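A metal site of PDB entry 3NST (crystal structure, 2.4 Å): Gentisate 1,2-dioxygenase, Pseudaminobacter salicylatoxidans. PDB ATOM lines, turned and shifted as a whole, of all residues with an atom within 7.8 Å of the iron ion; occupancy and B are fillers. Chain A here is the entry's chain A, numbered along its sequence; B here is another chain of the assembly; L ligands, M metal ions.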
ATOM      1  N   GLN A 108      25.560 -18.508  28.837  1.00  0.00           N
ATOM      2  CA  GLN A 108      24.374 -17.775  28.513  1.00  0.00           C
ATOM      3  C   GLN A 108      23.622 -17.500  29.762  1.00  0.00           C
ATOM      4  O   GLN A 108      23.397 -18.405  30.564  1.00  0.00           O
ATOM      5  CB  GLN A 108      23.474 -18.567  27.594  1.00  0.00           C
ATOM      6  CG  GLN A 108      22.221 -17.829  27.216  1.00  0.00           C
ATOM      7  CD  GLN A 108      22.196 -17.459  25.777  1.00  0.00           C
ATOM      8  OE1 GLN A 108      22.717 -18.173  24.908  1.00  0.00           O
ATOM      9  NE2 GLN A 108      21.559 -16.330  25.489  1.00  0.00           N
ATOM     10  N   PRO A 117      13.578 -15.433  19.474  1.00  0.00           N
ATOM     11  CA  PRO A 117      12.807 -16.082  18.390  1.00  0.00           C
ATOM     12  C   PRO A 117      13.623 -17.178  17.673  1.00  0.00           C
ATOM     13  O   PRO A 117      14.835 -17.359  17.948  1.00  0.00           O
ATOM     14  CB  PRO A 117      12.516 -14.936  17.425  1.00  0.00           C
ATOM     15  CG  PRO A 117      13.655 -13.950  17.636  1.00  0.00           C
ATOM     16  CD  PRO A 117      14.051 -14.072  19.092  1.00  0.00           C
ATOM     17  N   GLU A 118      12.970 -17.873  16.750  1.00  0.00           N
ATOM     18  CA  GLU A 118      13.570 -18.982  16.044  1.00  0.00           C
ATOM     19  C   GLU A 118      14.582 -18.578  14.956  1.00  0.00           C
ATOM     20  O   GLU A 118      14.394 -17.601  14.208  1.00  0.00           O
ATOM     21  CB  GLU A 118      12.499 -19.915  15.488  1.00  0.00           C
ATOM     22  CG  GLU A 118      11.735 -20.594  16.613  1.00  0.00           C
ATOM     23  CD  GLU A 118      10.645 -21.541  16.131  1.00  0.00           C
ATOM     24  OE1 GLU A 118      10.601 -21.916  14.902  1.00  0.00           O
ATOM     25  OE2 GLU A 118       9.822 -21.912  17.012  1.00  0.00           O
ATOM     26  N   HIS A 119      15.699 -19.316  14.930  1.00  0.00           N
ATOM     27  CA  HIS A 119      16.591 -19.303  13.775  1.00  0.00           C
ATOM     28  C   HIS A 119      17.183 -20.703  13.635  1.00  0.00           C
ATOM     29  O   HIS A 119      16.923 -21.573  14.459  1.00  0.00           O
ATOM     30  CB  HIS A 119      17.696 -18.255  13.969  1.00  0.00           C
ATOM     31  CG  HIS A 119      18.650 -18.593  15.065  1.00  0.00           C
ATOM     32  ND1 HIS A 119      19.102 -17.658  15.971  1.00  0.00           N
ATOM     33  CD2 HIS A 119      19.246 -19.755  15.404  1.00  0.00           C
ATOM     34  CE1 HIS A 119      19.939 -18.228  16.815  1.00  0.00           C
ATOM     35  NE2 HIS A 119      20.066 -19.506  16.478  1.00  0.00           N
ATOM     36  N   ARG A 120      17.922 -20.909  12.558  1.00  0.00           N
ATOM     37  CA  ARG A 120      18.714 -22.109  12.313  1.00  0.00           C
ATOM     38  C   ARG A 120      20.053 -21.681  11.684  1.00  0.00           C
ATOM     39  O   ARG A 120      20.176 -20.622  11.058  1.00  0.00           O
ATOM     40  CB  ARG A 120      17.976 -23.137  11.432  1.00  0.00           C
ATOM     41  CG  ARG A 120      17.096 -22.534  10.428  1.00  0.00           C
ATOM     42  CD  ARG A 120      17.059 -23.108   9.006  1.00  0.00           C
ATOM     43  NE  ARG A 120      16.401 -24.384   8.871  1.00  0.00           N
ATOM     44  CZ  ARG A 120      15.771 -24.817   7.762  1.00  0.00           C
ATOM     45  NH1 ARG A 120      15.246 -26.030   7.759  1.00  0.00           N
ATOM     46  NH2 ARG A 120      15.662 -24.068   6.656  1.00  0.00           N
ATOM     47  N   HIS A 121      21.058 -22.513  11.898  1.00  0.00           N
ATOM     48  CA  HIS A 121      22.386 -22.334  11.332  1.00  0.00           C
ATOM     49  C   HIS A 121      23.043 -23.732  11.197  1.00  0.00           C
ATOM     50  O   HIS A 121      22.721 -24.679  11.910  1.00  0.00           O
ATOM     51  CB  HIS A 121      23.223 -21.394  12.191  1.00  0.00           C
ATOM     52  CG  HIS A 121      23.023 -21.553  13.663  1.00  0.00           C
ATOM     53  ND1 HIS A 121      23.407 -22.692  14.365  1.00  0.00           N
ATOM     54  CD2 HIS A 121      22.509 -20.696  14.600  1.00  0.00           C
ATOM     55  CE1 HIS A 121      23.158 -22.523  15.654  1.00  0.00           C
ATOM     56  NE2 HIS A 121      22.602 -21.332  15.822  1.00  0.00           N
ATOM     57  N   GLN A 123      25.963 -24.511  11.946  1.00  0.00           N
ATOM     58  CA  GLN A 123      26.823 -24.794  13.107  1.00  0.00           C
ATOM     59  C   GLN A 123      26.054 -25.653  14.111  1.00  0.00           C
ATOM     60  O   GLN A 123      24.862 -25.377  14.331  1.00  0.00           O
ATOM     61  CB  GLN A 123      27.328 -23.514  13.774  1.00  0.00           C
ATOM     62  CG  GLN A 123      28.276 -22.629  12.863  1.00  0.00           C
ATOM     63  CD  GLN A 123      27.499 -21.689  11.888  1.00  0.00           C
ATOM     64  OE1 GLN A 123      26.340 -21.948  11.564  1.00  0.00           O
ATOM     65  NE2 GLN A 123      28.150 -20.580  11.450  1.00  0.00           N
ATOM     66  N   ALA A 125      25.138 -27.332  17.942  1.00  0.00           N
ATOM     67  CA  ALA A 125      25.111 -26.699  19.234  1.00  0.00           C
ATOM     68  C   ALA A 125      24.408 -27.532  20.299  1.00  0.00           C
ATOM     69  O   ALA A 125      23.461 -28.253  20.028  1.00  0.00           O
ATOM     70  CB  ALA A 125      24.434 -25.255  19.125  1.00  0.00           C
ATOM     71  N   ARG A 127      23.276 -27.125  24.774  1.00  0.00           N
ATOM     72  CA  ARG A 127      23.021 -26.239  25.902  1.00  0.00           C
ATOM     73  C   ARG A 127      22.988 -27.118  27.127  1.00  0.00           C
ATOM     74  O   ARG A 127      22.076 -27.948  27.258  1.00  0.00           O
ATOM     75  CB  ARG A 127      21.644 -25.568  25.764  1.00  0.00           C
ATOM     76  CG  ARG A 127      21.441 -24.878  24.455  1.00  0.00           C
ATOM     77  CD  ARG A 127      20.061 -24.256  24.358  1.00  0.00           C
ATOM     78  NE  ARG A 127      20.060 -23.290  23.254  1.00  0.00           N
ATOM     79  CZ  ARG A 127      19.134 -22.369  23.018  1.00  0.00           C
ATOM     80  NH1 ARG A 127      18.055 -22.285  23.808  1.00  0.00           N
ATOM     81  NH2 ARG A 127      19.278 -21.514  21.983  1.00  0.00           N
ATOM     82  N   THR A 154      20.735 -28.682  20.062  1.00  0.00           N
ATOM     83  CA  THR A 154      20.055 -28.088  18.934  1.00  0.00           C
ATOM     84  C   THR A 154      20.884 -28.341  17.671  1.00  0.00           C
ATOM     85  O   THR A 154      21.637 -27.490  17.225  1.00  0.00           O
ATOM     86  CB  THR A 154      19.727 -26.567  19.161  1.00  0.00           C
ATOM     87  OG1 THR A 154      20.965 -25.837  19.291  1.00  0.00           O
ATOM     88  CG2 THR A 154      18.882 -26.365  20.445  1.00  0.00           C
ATOM     89  N   CYS A 158      18.484 -27.140  12.594  1.00  0.00           N
ATOM     90  CA  CYS A 158      17.226 -27.253  13.325  1.00  0.00           C
ATOM     91  C   CYS A 158      16.839 -25.882  13.843  1.00  0.00           C
ATOM     92  O   CYS A 158      17.630 -25.223  14.500  1.00  0.00           O
ATOM     93  CB  CYS A 158      17.365 -28.189  14.545  1.00  0.00           C
ATOM     94  SG  CYS A 158      17.642 -29.953  14.096  1.00  0.00           S
ATOM     95  N   PHE A 159      15.587 -25.487  13.608  1.00  0.00           N
ATOM     96  CA  PHE A 159      15.112 -24.205  14.179  1.00  0.00           C
ATOM     97  C   PHE A 159      15.172 -24.280  15.693  1.00  0.00           C
ATOM     98  O   PHE A 159      14.842 -25.314  16.271  1.00  0.00           O
ATOM     99  CB  PHE A 159      13.682 -23.854  13.662  1.00  0.00           C
ATOM    100  CG  PHE A 159      13.666 -23.324  12.243  1.00  0.00           C
ATOM    101  CD1 PHE A 159      13.187 -24.125  11.194  1.00  0.00           C
ATOM    102  CD2 PHE A 159      14.151 -22.026  11.948  1.00  0.00           C
ATOM    103  CE1 PHE A 159      13.171 -23.663   9.855  1.00  0.00           C
ATOM    104  CE2 PHE A 159      14.131 -21.518  10.612  1.00  0.00           C
ATOM    105  CZ  PHE A 159      13.617 -22.356   9.547  1.00  0.00           C
ATOM    106  N   HIS A 160      15.682 -23.233  16.336  1.00  0.00           N
ATOM    107  CA  HIS A 160      15.611 -23.170  17.786  1.00  0.00           C
ATOM    108  C   HIS A 160      15.343 -21.744  18.311  1.00  0.00           C
ATOM    109  O   HIS A 160      16.060 -20.803  17.972  1.00  0.00           O
ATOM    110  CB  HIS A 160      16.844 -23.799  18.456  1.00  0.00           C
ATOM    111  CG  HIS A 160      18.140 -23.209  18.002  1.00  0.00           C
ATOM    112  ND1 HIS A 160      18.716 -23.532  16.793  1.00  0.00           N
ATOM    113  CD2 HIS A 160      18.968 -22.300  18.577  1.00  0.00           C
ATOM    114  CE1 HIS A 160      19.857 -22.861  16.647  1.00  0.00           C
ATOM    115  NE2 HIS A 160      20.032 -22.099  17.714  1.00  0.00           N
ATOM    116  N   GLY A 161      14.316 -21.593  19.159  1.00  0.00           N
ATOM    117  CA  GLY A 161      14.185 -20.396  19.977  1.00  0.00           C
ATOM    118  C   GLY A 161      13.959 -20.848  21.403  1.00  0.00           C
ATOM    119  O   GLY A 161      13.925 -22.018  21.674  1.00  0.00           O
ATOM    120  N   ASP A 174      26.667 -22.655  26.543  1.00  0.00           N
ATOM    121  CA  ASP A 174      26.207 -22.541  25.191  1.00  0.00           C
ATOM    122  C   ASP A 174      27.406 -23.055  24.380  1.00  0.00           C
ATOM    123  O   ASP A 174      28.421 -22.323  24.290  1.00  0.00           O
ATOM    124  CB  ASP A 174      25.989 -21.058  24.958  1.00  0.00           C
ATOM    125  CG  ASP A 174      25.524 -20.708  23.534  1.00  0.00           C
ATOM    126  OD1 ASP A 174      26.102 -19.749  22.907  1.00  0.00           O
ATOM    127  OD2 ASP A 174      24.531 -21.346  23.069  1.00  0.00           O
ATOM    128  N   LEU A 176      29.275 -24.629  20.889  1.00  0.00           N
ATOM    129  CA  LEU A 176      29.124 -24.758  19.453  1.00  0.00           C
ATOM    130  C   LEU A 176      30.446 -25.015  18.695  1.00  0.00           C
ATOM    131  O   LEU A 176      31.537 -24.806  19.268  1.00  0.00           O
ATOM    132  CB  LEU A 176      28.457 -23.531  18.825  1.00  0.00           C
ATOM    133  CG  LEU A 176      27.047 -23.145  19.216  1.00  0.00           C
ATOM    134  CD1 LEU A 176      27.120 -22.067  20.341  1.00  0.00           C
ATOM    135  CD2 LEU A 176      26.412 -22.613  17.993  1.00  0.00           C
ATOM    136  N   ILE A 178      31.377 -23.204  16.322  1.00  0.00           N
ATOM    137  CA  ILE A 178      31.527 -21.882  15.640  1.00  0.00           C
ATOM    138  C   ILE A 178      32.919 -21.628  15.044  1.00  0.00           C
ATOM    139  O   ILE A 178      33.000 -21.233  13.857  1.00  0.00           O
ATOM    140  CB  ILE A 178      31.054 -20.674  16.554  1.00  0.00           C
ATOM    141  CG1 ILE A 178      29.539 -20.396  16.350  1.00  0.00           C
ATOM    142  CG2 ILE A 178      31.834 -19.406  16.292  1.00  0.00           C
ATOM    143  CD1 ILE A 178      28.933 -19.594  17.569  1.00  0.00           C
ATOM    144  N   PHE A 189      22.936 -19.495   7.718  1.00  0.00           N
ATOM    145  CA  PHE A 189      22.094 -18.936   8.766  1.00  0.00           C
ATOM    146  C   PHE A 189      20.772 -18.408   8.221  1.00  0.00           C
ATOM    147  O   PHE A 189      20.753 -17.702   7.201  1.00  0.00           O
ATOM    148  CB  PHE A 189      22.849 -17.834   9.470  1.00  0.00           C
ATOM    149  CG  PHE A 189      22.150 -17.317  10.647  1.00  0.00           C
ATOM    150  CD1 PHE A 189      20.987 -16.543  10.497  1.00  0.00           C
ATOM    151  CD2 PHE A 189      22.625 -17.603  11.914  1.00  0.00           C
ATOM    152  CE1 PHE A 189      20.294 -16.054  11.623  1.00  0.00           C
ATOM    153  CE2 PHE A 189      21.960 -17.128  13.047  1.00  0.00           C
ATOM    154  CZ  PHE A 189      20.799 -16.357  12.911  1.00  0.00           C
ATOM    155  N   MET B  46      28.605 -15.898  12.515  1.00  0.00           N
ATOM    156  CA  MET B  46      27.673 -16.873  11.957  1.00  0.00           C
ATOM    157  C   MET B  46      27.029 -16.314  10.654  1.00  0.00           C
ATOM    158  O   MET B  46      25.897 -15.848  10.613  1.00  0.00           O
ATOM    159  CB  MET B  46      26.570 -17.303  12.980  1.00  0.00           C
ATOM    160  CG  MET B  46      27.035 -17.684  14.396  1.00  0.00           C
ATOM    161  SD  MET B  46      25.759 -18.514  15.439  1.00  0.00           S
ATOM    162  CE  MET B  46      25.742 -20.151  14.744  1.00  0.00           C
HETATM  163  C1  LIG L   1      21.965 -19.141  20.520  1.00  0.00           C
HETATM  164  O1  LIG L   1      21.006 -19.745  19.646  1.00  0.00           O
HETATM  165  C2  LIG L   1      23.399 -19.627  20.206  1.00  0.00           C
HETATM  166  O2  LIG L   1      24.508 -18.737  20.400  1.00  0.00           O
HETATM  167  C3  LIG L   1      23.616 -20.761  19.219  1.00  0.00           C
HETATM  168  O3  LIG L   1      22.663 -21.740  19.500  1.00  0.00           O
HETATM  169 FE    FE M   1      21.491 -20.541  17.642  1.00  0.00          FE
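The iron ion is bound by NE2 of His 119 (2.1 Å), NE2 of His 160 (2.1 Å), O1 of the ligand (2.2 Å), NE2 of His 121 (2.3 Å) and O3 of the ligand (2.5 Å). The iron ion has five donor atoms within binding distance.
Three residues have an atom within 4 Å of the iron ion: His 119, His 121 and His 160. The nearest printed residue that does not touch the iron ion is Arg 127 (5.0 Å).
A ring nitrogen (ND1) of His 160 sits at hydrogen-bond distance from the backbone carbonyl oxygen (O) of Cys 158 (3.0 Å). ND1 of His 121 is in hydrogen-bond range of O of Gln 123, at 3.1 Å.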
